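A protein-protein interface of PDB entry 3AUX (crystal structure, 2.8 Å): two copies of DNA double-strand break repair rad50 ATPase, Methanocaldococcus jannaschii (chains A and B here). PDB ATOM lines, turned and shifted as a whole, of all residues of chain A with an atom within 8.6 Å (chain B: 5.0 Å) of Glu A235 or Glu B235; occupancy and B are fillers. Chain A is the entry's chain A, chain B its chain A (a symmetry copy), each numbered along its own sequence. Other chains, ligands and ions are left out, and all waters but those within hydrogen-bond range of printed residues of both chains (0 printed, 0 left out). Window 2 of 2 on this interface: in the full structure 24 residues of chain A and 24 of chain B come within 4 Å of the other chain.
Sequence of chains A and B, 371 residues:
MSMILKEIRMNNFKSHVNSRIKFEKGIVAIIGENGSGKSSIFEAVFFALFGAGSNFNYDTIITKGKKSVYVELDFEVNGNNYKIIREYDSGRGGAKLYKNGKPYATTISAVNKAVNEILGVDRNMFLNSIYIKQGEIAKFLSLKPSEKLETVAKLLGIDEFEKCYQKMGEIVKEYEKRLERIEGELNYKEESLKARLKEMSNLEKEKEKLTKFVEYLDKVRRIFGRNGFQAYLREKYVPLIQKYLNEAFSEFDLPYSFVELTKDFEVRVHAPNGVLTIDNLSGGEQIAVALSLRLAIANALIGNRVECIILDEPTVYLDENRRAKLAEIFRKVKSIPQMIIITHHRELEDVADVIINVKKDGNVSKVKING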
ATOM      1  N   LEU A 156       0.641  31.574  -1.755  1.00  0.00           N
ATOM      2  CA  LEU A 156       0.533  31.810  -3.192  1.00  0.00           C
ATOM      3  C   LEU A 156      -0.716  32.635  -3.535  1.00  0.00           C
ATOM      4  O   LEU A 156      -0.814  33.216  -4.621  1.00  0.00           O
ATOM      5  CB  LEU A 156       0.524  30.472  -3.946  1.00  0.00           C
ATOM      6  CG  LEU A 156       1.869  29.778  -4.207  1.00  0.00           C
ATOM      7  CD1 LEU A 156       2.660  29.675  -2.931  1.00  0.00           C
ATOM      8  CD2 LEU A 156       1.636  28.399  -4.780  1.00  0.00           C
ATOM      9  N   ILE A 158      -4.006  31.490  -3.708  1.00  0.00           N
ATOM     10  CA  ILE A 158      -4.999  30.776  -4.500  1.00  0.00           C
ATOM     11  C   ILE A 158      -6.457  31.251  -4.326  1.00  0.00           C
ATOM     12  O   ILE A 158      -7.316  30.946  -5.160  1.00  0.00           O
ATOM     13  CB  ILE A 158      -4.883  29.253  -4.235  1.00  0.00           C
ATOM     14  CG1 ILE A 158      -3.663  28.714  -4.984  1.00  0.00           C
ATOM     15  CG2 ILE A 158      -6.144  28.524  -4.658  1.00  0.00           C
ATOM     16  CD1 ILE A 158      -3.532  27.215  -4.946  1.00  0.00           C
ATOM     17  N   GLY A 228     -10.811  27.500 -12.779  1.00  0.00           N
ATOM     18  CA  GLY A 228      -9.676  27.161 -13.615  1.00  0.00           C
ATOM     19  C   GLY A 228      -8.462  27.992 -13.249  1.00  0.00           C
ATOM     20  O   GLY A 228      -7.327  27.618 -13.551  1.00  0.00           O
ATOM     21  N   PHE A 229      -8.708  29.120 -12.584  1.00  0.00           N
ATOM     22  CA  PHE A 229      -7.645  30.031 -12.176  1.00  0.00           C
ATOM     23  C   PHE A 229      -6.670  29.387 -11.204  1.00  0.00           C
ATOM     24  O   PHE A 229      -5.510  29.791 -11.126  1.00  0.00           O
ATOM     25  CB  PHE A 229      -8.239  31.281 -11.541  1.00  0.00           C
ATOM     26  CG  PHE A 229      -7.271  32.416 -11.437  1.00  0.00           C
ATOM     27  CD1 PHE A 229      -6.592  32.864 -12.563  1.00  0.00           C
ATOM     28  CD2 PHE A 229      -7.055  33.057 -10.223  1.00  0.00           C
ATOM     29  CE1 PHE A 229      -5.712  33.941 -12.482  1.00  0.00           C
ATOM     30  CE2 PHE A 229      -6.175  34.137 -10.129  1.00  0.00           C
ATOM     31  CZ  PHE A 229      -5.503  34.579 -11.260  1.00  0.00           C
ATOM     32  N   GLN A 230      -7.146  28.395 -10.456  1.00  0.00           N
ATOM     33  CA  GLN A 230      -6.303  27.681  -9.504  1.00  0.00           C
ATOM     34  C   GLN A 230      -5.477  26.652 -10.265  1.00  0.00           C
ATOM     35  O   GLN A 230      -4.268  26.540 -10.068  1.00  0.00           O
ATOM     36  CB  GLN A 230      -7.153  26.965  -8.460  1.00  0.00           C
ATOM     37  CG  GLN A 230      -8.152  27.855  -7.767  1.00  0.00           C
ATOM     38  CD  GLN A 230      -8.845  27.142  -6.628  1.00  0.00           C
ATOM     39  OE1 GLN A 230      -9.330  26.020  -6.788  1.00  0.00           O
ATOM     40  NE2 GLN A 230      -8.901  27.792  -5.470  1.00  0.00           N
ATOM     41  N   ALA A 231      -6.138  25.899 -11.135  1.00  0.00           N
ATOM     42  CA  ALA A 231      -5.461  24.888 -11.936  1.00  0.00           C
ATOM     43  C   ALA A 231      -4.292  25.548 -12.652  1.00  0.00           C
ATOM     44  O   ALA A 231      -3.312  24.891 -13.006  1.00  0.00           O
ATOM     45  CB  ALA A 231      -6.432  24.289 -12.950  1.00  0.00           C
ATOM     46  N   TYR A 232      -4.409  26.859 -12.854  1.00  0.00           N
ATOM     47  CA  TYR A 232      -3.377  27.640 -13.526  1.00  0.00           C
ATOM     48  C   TYR A 232      -2.202  27.951 -12.604  1.00  0.00           C
ATOM     49  O   TYR A 232      -1.058  27.589 -12.891  1.00  0.00           O
ATOM     50  CB  TYR A 232      -3.961  28.957 -14.054  1.00  0.00           C
ATOM     51  CG  TYR A 232      -2.915  29.898 -14.618  1.00  0.00           C
ATOM     52  CD1 TYR A 232      -2.051  29.481 -15.633  1.00  0.00           C
ATOM     53  CD2 TYR A 232      -2.761  31.190 -14.114  1.00  0.00           C
ATOM     54  CE1 TYR A 232      -1.054  30.325 -16.130  1.00  0.00           C
ATOM     55  CE2 TYR A 232      -1.768  32.042 -14.605  1.00  0.00           C
ATOM     56  CZ  TYR A 232      -0.919  31.601 -15.611  1.00  0.00           C
ATOM     57  OH  TYR A 232       0.071  32.426 -16.097  1.00  0.00           O
ATOM     58  N   LEU A 233      -2.500  28.635 -11.503  1.00  0.00           N
ATOM     59  CA  LEU A 233      -1.489  29.013 -10.531  1.00  0.00           C
ATOM     60  C   LEU A 233      -0.561  27.854 -10.183  1.00  0.00           C
ATOM     61  O   LEU A 233       0.648  28.044 -10.046  1.00  0.00           O
ATOM     62  CB  LEU A 233      -2.162  29.561  -9.273  1.00  0.00           C
ATOM     63  CG  LEU A 233      -3.018  30.809  -9.520  1.00  0.00           C
ATOM     64  CD1 LEU A 233      -3.609  31.314  -8.205  1.00  0.00           C
ATOM     65  CD2 LEU A 233      -2.165  31.887 -10.172  1.00  0.00           C
ATOM     66  N   ARG A 234      -1.118  26.654 -10.051  1.00  0.00           N
ATOM     67  CA  ARG A 234      -0.314  25.475  -9.735  1.00  0.00           C
ATOM     68  C   ARG A 234       0.666  25.198 -10.868  1.00  0.00           C
ATOM     69  O   ARG A 234       1.695  24.556 -10.673  1.00  0.00           O
ATOM     70  CB  ARG A 234      -1.211  24.251  -9.539  1.00  0.00           C
ATOM     71  CG  ARG A 234      -2.239  24.397  -8.433  1.00  0.00           C
ATOM     72  CD  ARG A 234      -3.276  23.289  -8.502  1.00  0.00           C
ATOM     73  NE  ARG A 234      -4.332  23.476  -7.516  1.00  0.00           N
ATOM     74  CZ  ARG A 234      -4.204  23.199  -6.224  1.00  0.00           C
ATOM     75  NH1 ARG A 234      -3.064  22.710  -5.754  1.00  0.00           N
ATOM     76  NH2 ARG A 234      -5.215  23.423  -5.402  1.00  0.00           N
ATOM     77  N   GLU A 235       0.332  25.685 -12.057  1.00  0.00           N
ATOM     78  CA  GLU A 235       1.165  25.486 -13.235  1.00  0.00           C
ATOM     79  C   GLU A 235       2.290  26.508 -13.292  1.00  0.00           C
ATOM     80  O   GLU A 235       3.410  26.198 -13.711  1.00  0.00           O
ATOM     81  CB  GLU A 235       0.314  25.608 -14.501  1.00  0.00           C
ATOM     82  CG  GLU A 235      -0.865  24.651 -14.560  1.00  0.00           C
ATOM     83  CD  GLU A 235      -0.445  23.200 -14.414  1.00  0.00           C
ATOM     84  OE1 GLU A 235       0.584  22.813 -15.020  1.00  0.00           O
ATOM     85  OE2 GLU A 235      -1.147  22.447 -13.701  1.00  0.00           O
ATOM     86  N   LYS A 236       1.972  27.726 -12.868  1.00  0.00           N
ATOM     87  CA  LYS A 236       2.925  28.828 -12.865  1.00  0.00           C
ATOM     88  C   LYS A 236       3.950  28.748 -11.736  1.00  0.00           C
ATOM     89  O   LYS A 236       5.154  28.851 -11.975  1.00  0.00           O
ATOM     90  CB  LYS A 236       2.175  30.166 -12.766  1.00  0.00           C
ATOM     91  CG  LYS A 236       3.082  31.388 -12.755  1.00  0.00           C
ATOM     92  CD  LYS A 236       2.319  32.673 -12.480  1.00  0.00           C
ATOM     93  CE  LYS A 236       3.272  33.858 -12.510  1.00  0.00           C
ATOM     94  NZ  LYS A 236       2.633  35.150 -12.142  1.00  0.00           N
ATOM     95  N   TYR A 237       3.463  28.552 -10.512  1.00  0.00           N
ATOM     96  CA  TYR A 237       4.321  28.515  -9.337  1.00  0.00           C
ATOM     97  C   TYR A 237       5.101  27.232  -9.068  1.00  0.00           C
ATOM     98  O   TYR A 237       6.333  27.261  -9.018  1.00  0.00           O
ATOM     99  CB  TYR A 237       3.507  28.885  -8.096  1.00  0.00           C
ATOM    100  CG  TYR A 237       2.875  30.263  -8.147  1.00  0.00           C
ATOM    101  CD1 TYR A 237       3.573  31.363  -8.648  1.00  0.00           C
ATOM    102  CD2 TYR A 237       1.591  30.474  -7.656  1.00  0.00           C
ATOM    103  CE1 TYR A 237       3.002  32.638  -8.654  1.00  0.00           C
ATOM    104  CE2 TYR A 237       1.014  31.741  -7.654  1.00  0.00           C
ATOM    105  CZ  TYR A 237       1.721  32.820  -8.151  1.00  0.00           C
ATOM    106  OH  TYR A 237       1.139  34.073  -8.124  1.00  0.00           O
ATOM    107  N   VAL A 238       4.397  26.120  -8.878  1.00  0.00           N
ATOM    108  CA  VAL A 238       5.048  24.837  -8.597  1.00  0.00           C
ATOM    109  C   VAL A 238       6.376  24.666  -9.330  1.00  0.00           C
ATOM    110  O   VAL A 238       7.409  24.370  -8.718  1.00  0.00           O
ATOM    111  CB  VAL A 238       4.135  23.638  -8.966  1.00  0.00           C
ATOM    112  CG1 VAL A 238       4.886  22.324  -8.756  1.00  0.00           C
ATOM    113  CG2 VAL A 238       2.869  23.663  -8.122  1.00  0.00           C
ATOM    114  N   PRO A 239       6.370  24.841 -10.658  1.00  0.00           N
ATOM    115  CA  PRO A 239       7.642  24.677 -11.372  1.00  0.00           C
ATOM    116  C   PRO A 239       8.736  25.536 -10.723  1.00  0.00           C
ATOM    117  O   PRO A 239       9.819  25.035 -10.389  1.00  0.00           O
ATOM    118  CB  PRO A 239       7.296  25.126 -12.792  1.00  0.00           C
ATOM    119  CG  PRO A 239       5.834  24.739 -12.913  1.00  0.00           C
ATOM    120  CD  PRO A 239       5.280  25.197 -11.587  1.00  0.00           C
ATOM    121  N   LEU A 240       8.417  26.821 -10.535  1.00  0.00           N
ATOM    122  CA  LEU A 240       9.318  27.804  -9.931  1.00  0.00           C
ATOM    123  C   LEU A 240       9.790  27.396  -8.549  1.00  0.00           C
ATOM    124  O   LEU A 240      10.996  27.267  -8.305  1.00  0.00           O
ATOM    125  CB  LEU A 240       8.623  29.157  -9.827  1.00  0.00           C
ATOM    126  CG  LEU A 240       8.320  29.824 -11.164  1.00  0.00           C
ATOM    127  CD1 LEU A 240       7.542  31.114 -10.946  1.00  0.00           C
ATOM    128  CD2 LEU A 240       9.628  30.087 -11.889  1.00  0.00           C
ATOM    129  N   ILE A 241       8.832  27.203  -7.644  1.00  0.00           N
ATOM    130  CA  ILE A 241       9.148  26.817  -6.283  1.00  0.00           C
ATOM    131  C   ILE A 241      10.093  25.625  -6.245  1.00  0.00           C
ATOM    132  O   ILE A 241      11.062  25.638  -5.494  1.00  0.00           O
ATOM    133  CB  ILE A 241       7.876  26.476  -5.483  1.00  0.00           C
ATOM    134  CG1 ILE A 241       6.925  27.668  -5.483  1.00  0.00           C
ATOM    135  CG2 ILE A 241       8.234  26.132  -4.046  1.00  0.00           C
ATOM    136  CD1 ILE A 241       5.690  27.432  -4.649  1.00  0.00           C
ATOM    137  N   THR A 262       5.003  18.376  -5.635  1.00  0.00           N
ATOM    138  CA  THR A 262       3.768  17.968  -6.302  1.00  0.00           C
ATOM    139  C   THR A 262       2.910  19.177  -6.626  1.00  0.00           C
ATOM    140  O   THR A 262       3.146  20.269  -6.106  1.00  0.00           O
ATOM    141  CB  THR A 262       2.927  17.025  -5.423  1.00  0.00           C
ATOM    142  OG1 THR A 262       2.117  17.800  -4.530  1.00  0.00           O
ATOM    143  CG2 THR A 262       3.830  16.094  -4.619  1.00  0.00           C
ATOM    144  N   LYS A 263       1.913  18.982  -7.485  1.00  0.00           N
ATOM    145  CA  LYS A 263       1.025  20.075  -7.857  1.00  0.00           C
ATOM    146  C   LYS A 263       0.050  20.383  -6.731  1.00  0.00           C
ATOM    147  O   LYS A 263      -0.836  21.227  -6.871  1.00  0.00           O
ATOM    148  CB  LYS A 263       0.270  19.751  -9.148  1.00  0.00           C
ATOM    149  CG  LYS A 263       0.936  20.321 -10.410  1.00  0.00           C
ATOM    150  CD  LYS A 263       0.148  19.977 -11.666  1.00  0.00           C
ATOM    151  CE  LYS A 263      -1.308  20.440 -11.546  1.00  0.00           C
ATOM    152  NZ  LYS A 263      -2.163  19.923 -12.655  1.00  0.00           N
ATOM    153  N   PHE A 265       1.474  20.857  -3.693  1.00  0.00           N
ATOM    154  CA  PHE A 265       2.429  21.508  -2.798  1.00  0.00           C
ATOM    155  C   PHE A 265       3.053  20.596  -1.750  1.00  0.00           C
ATOM    156  O   PHE A 265       3.403  21.059  -0.665  1.00  0.00           O
ATOM    157  CB  PHE A 265       1.770  22.703  -2.100  1.00  0.00           C
ATOM    158  CG  PHE A 265       1.056  23.626  -3.040  1.00  0.00           C
ATOM    159  CD1 PHE A 265       1.726  24.196  -4.118  1.00  0.00           C
ATOM    160  CD2 PHE A 265      -0.293  23.911  -2.860  1.00  0.00           C
ATOM    161  CE1 PHE A 265       1.060  25.040  -5.003  1.00  0.00           C
ATOM    162  CE2 PHE A 265      -0.968  24.750  -3.736  1.00  0.00           C
ATOM    163  CZ  PHE A 265      -0.292  25.316  -4.810  1.00  0.00           C
ATOM    164  N   ALA B 231       0.364  28.346 -21.461  1.00  0.00           N
ATOM    165  CA  ALA B 231       0.678  27.270 -20.531  1.00  0.00           C
ATOM    166  C   ALA B 231      -0.607  26.853 -19.830  1.00  0.00           C
ATOM    167  O   ALA B 231      -0.736  25.720 -19.365  1.00  0.00           O
ATOM    168  CB  ALA B 231       1.706  27.747 -19.510  1.00  0.00           C
ATOM    169  N   TYR B 232      -1.555  27.785 -19.767  1.00  0.00           N
ATOM    170  CA  TYR B 232      -2.845  27.545 -19.129  1.00  0.00           C
ATOM    171  C   TYR B 232      -3.783  26.740 -20.020  1.00  0.00           C
ATOM    172  O   TYR B 232      -4.243  25.658 -19.643  1.00  0.00           O
ATOM    173  CB  TYR B 232      -3.517  28.876 -18.765  1.00  0.00           C
ATOM    174  CG  TYR B 232      -4.933  28.714 -18.249  1.00  0.00           C
ATOM    175  CD1 TYR B 232      -5.207  27.887 -17.157  1.00  0.00           C
ATOM    176  CD2 TYR B 232      -6.005  29.354 -18.873  1.00  0.00           C
ATOM    177  CE1 TYR B 232      -6.513  27.697 -16.700  1.00  0.00           C
ATOM    178  CE2 TYR B 232      -7.315  29.171 -18.424  1.00  0.00           C
ATOM    179  CZ  TYR B 232      -7.561  28.339 -17.338  1.00  0.00           C
ATOM    180  OH  TYR B 232      -8.847  28.142 -16.892  1.00  0.00           O
ATOM    181  N   LEU B 233      -4.071  27.288 -21.197  1.00  0.00           N
ATOM    182  CA  LEU B 233      -4.957  26.645 -22.153  1.00  0.00           C
ATOM    183  C   LEU B 233      -4.632  25.167 -22.337  1.00  0.00           C
ATOM    184  O   LEU B 233      -5.537  24.338 -22.434  1.00  0.00           O
ATOM    185  CB  LEU B 233      -4.894  27.381 -23.490  1.00  0.00           C
ATOM    186  CG  LEU B 233      -5.327  28.850 -23.412  1.00  0.00           C
ATOM    187  CD1 LEU B 233      -5.280  29.491 -24.798  1.00  0.00           C
ATOM    188  CD2 LEU B 233      -6.731  28.933 -22.833  1.00  0.00           C
ATOM    189  N   ARG B 234      -3.346  24.832 -22.374  1.00  0.00           N
ATOM    190  CA  ARG B 234      -2.929  23.439 -22.531  1.00  0.00           C
ATOM    191  C   ARG B 234      -3.389  22.623 -21.330  1.00  0.00           C
ATOM    192  O   ARG B 234      -3.535  21.406 -21.410  1.00  0.00           O
ATOM    193  CB  ARG B 234      -1.405  23.346 -22.644  1.00  0.00           C
ATOM    194  CG  ARG B 234      -0.816  24.120 -23.808  1.00  0.00           C
ATOM    195  CD  ARG B 234       0.695  24.233 -23.677  1.00  0.00           C
ATOM    196  NE  ARG B 234       1.266  25.068 -24.727  1.00  0.00           N
ATOM    197  CZ  ARG B 234       1.460  24.664 -25.976  1.00  0.00           C
ATOM    198  NH1 ARG B 234       1.140  23.429 -26.339  1.00  0.00           N
ATOM    199  NH2 ARG B 234       1.967  25.502 -26.864  1.00  0.00           N
ATOM    200  N   GLU B 235      -3.611  23.306 -20.213  1.00  0.00           N
ATOM    201  CA  GLU B 235      -4.041  22.657 -18.982  1.00  0.00           C
ATOM    202  C   GLU B 235      -5.545  22.434 -18.975  1.00  0.00           C
ATOM    203  O   GLU B 235      -6.035  21.418 -18.475  1.00  0.00           O
ATOM    204  CB  GLU B 235      -3.656  23.519 -17.777  1.00  0.00           C
ATOM    205  CG  GLU B 235      -2.174  23.836 -17.679  1.00  0.00           C
ATOM    206  CD  GLU B 235      -1.313  22.586 -17.658  1.00  0.00           C
ATOM    207  OE1 GLU B 235      -1.694  21.611 -16.967  1.00  0.00           O
ATOM    208  OE2 GLU B 235      -0.252  22.586 -18.324  1.00  0.00           O
ATOM    209  N   LYS B 236      -6.265  23.400 -19.535  1.00  0.00           N
ATOM    210  CA  LYS B 236      -7.720  23.354 -19.603  1.00  0.00           C
ATOM    211  C   LYS B 236      -8.253  22.399 -20.668  1.00  0.00           C
ATOM    212  O   LYS B 236      -9.105  21.557 -20.383  1.00  0.00           O
ATOM    213  CB  LYS B 236      -8.274  24.762 -19.873  1.00  0.00           C
ATOM    214  CG  LYS B 236      -9.791  24.827 -19.963  1.00  0.00           C
ATOM    215  CD  LYS B 236     -10.288  26.194 -20.403  1.00  0.00           C
ATOM    216  CE  LYS B 236     -11.809  26.203 -20.447  1.00  0.00           C
ATOM    217  NZ  LYS B 236     -12.384  27.470 -20.974  1.00  0.00           N
ATOM    218  N   TYR B 237      -7.734  22.529 -21.888  1.00  0.00           N
ATOM    219  CA  TYR B 237      -8.193  21.723 -23.011  1.00  0.00           C
ATOM    220  C   TYR B 237      -7.683  20.290 -23.111  1.00  0.00           C
ATOM    221  O   TYR B 237      -8.482  19.352 -23.105  1.00  0.00           O
ATOM    222  CB  TYR B 237      -7.904  22.459 -24.321  1.00  0.00           C
ATOM    223  CG  TYR B 237      -8.571  23.817 -24.439  1.00  0.00           C
ATOM    224  CD1 TYR B 237      -9.886  24.017 -24.019  1.00  0.00           C
ATOM    225  CD2 TYR B 237      -7.897  24.891 -25.010  1.00  0.00           C
ATOM    226  CE1 TYR B 237     -10.511  25.259 -24.168  1.00  0.00           C
ATOM    227  CE2 TYR B 237      -8.511  26.131 -25.167  1.00  0.00           C
ATOM    228  CZ  TYR B 237      -9.815  26.312 -24.748  1.00  0.00           C
ATOM    229  OH  TYR B 237     -10.415  27.543 -24.930  1.00  0.00           O
ATOM    230  N   VAL B 238      -6.368  20.118 -23.222  1.00  0.00           N
ATOM    231  CA  VAL B 238      -5.776  18.782 -23.340  1.00  0.00           C
ATOM    232  C   VAL B 238      -6.519  17.723 -22.531  1.00  0.00           C
ATOM    233  O   VAL B 238      -6.916  16.678 -23.059  1.00  0.00           O
ATOM    234  CB  VAL B 238      -4.289  18.773 -22.896  1.00  0.00           C
ATOM    235  CG1 VAL B 238      -3.739  17.348 -22.937  1.00  0.00           C
ATOM    236  CG2 VAL B 238      -3.467  19.682 -23.798  1.00  0.00           C
ATOM    237  N   PRO B 239      -6.715  17.972 -21.229  1.00  0.00           N
ATOM    238  CA  PRO B 239      -7.427  16.958 -20.443  1.00  0.00           C
ATOM    239  C   PRO B 239      -8.752  16.585 -21.121  1.00  0.00           C
ATOM    240  O   PRO B 239      -9.034  15.401 -21.351  1.00  0.00           O
ATOM    241  CB  PRO B 239      -7.624  17.650 -19.093  1.00  0.00           C
ATOM    242  CG  PRO B 239      -6.404  18.549 -19.003  1.00  0.00           C
ATOM    243  CD  PRO B 239      -6.344  19.130 -20.395  1.00  0.00           C
ATOM    244  N   LYS B 263       0.786  17.421 -24.004  1.00  0.00           N
ATOM    245  CA  LYS B 263       0.485  18.831 -23.788  1.00  0.00           C
ATOM    246  C   LYS B 263       0.918  19.664 -24.984  1.00  0.00           C
ATOM    247  O   LYS B 263       0.821  20.892 -24.973  1.00  0.00           O
ATOM    248  CB  LYS B 263       1.152  19.342 -22.509  1.00  0.00           C
ATOM    249  CG  LYS B 263       0.230  19.312 -21.280  1.00  0.00           C
ATOM    250  CD  LYS B 263       0.934  19.832 -20.035  1.00  0.00           C
ATOM    251  CE  LYS B 263       1.504  21.234 -20.271  1.00  0.00           C
ATOM    252  NZ  LYS B 263       2.391  21.683 -19.157  1.00  0.00           N
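Tyr A232 touches its own counterpart, Tyr B232. Glu B235 touches its own counterpart, Glu A235. Positions printed for both chains: 231, 232, 233, 234, 235, 236, 237, 238, 239 and 263. Of the 3 pairs that touch across the chains among the printed residues, 2 have their exchanged pair printed and touching as well.
Of the 19 printed residues of chain A, 3 touch a printed residue of chain B. Printed residues of chain A that touch a printed residue of chain B: Gly A228, Tyr A232 and Glu A235. Hydrophobic or aromatic side chains of chain A that line the printed part of chain B: Tyr A232. Of the 10 printed residues of chain B, 2 touch a printed residue of chain A. Hydrophobic or aromatic side chains of chain B within 4 Å of the printed part of chain A: Tyr B232. Among the printed residues, 3 pairs touch across the chains.
The side-chain amino group (NZ) of Lys A263 lies within salt-bridge range of the side-chain carboxylate (OE2) of Glu A235. OE2 of Glu B235 lies within salt-bridge range of NZ of Lys B263 (2.9 Å).
Among the printed residues, pairs that only touch across the chains: Gly A228 with Tyr B232 and Tyr A232 with Tyr B232.
Of the printed residues of chain B, Gly A228 touches Tyr B232 (3.3 Å). Of the printed residues of chain B, Tyr A232 touches Tyr B232 (3.5 Å). Of chain B, only Glu B235 comes within 4 Å of Glu A235. Of the printed residues of chain A, Tyr B232 touches Gly A228 (3.3 Å) and Tyr A232 (3.5 Å). Glu B235 touches one residue of chain A. The nearest residue of chain B that does not touch Glu A235 is Lys B263 (4.7 Å). The nearest printed residue of chain B that does not touch Gly A228 is Lys B236 (6.8 Å).
OE1 of Glu B235 sits close to OE1 of Glu A235 (3.2 Å).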
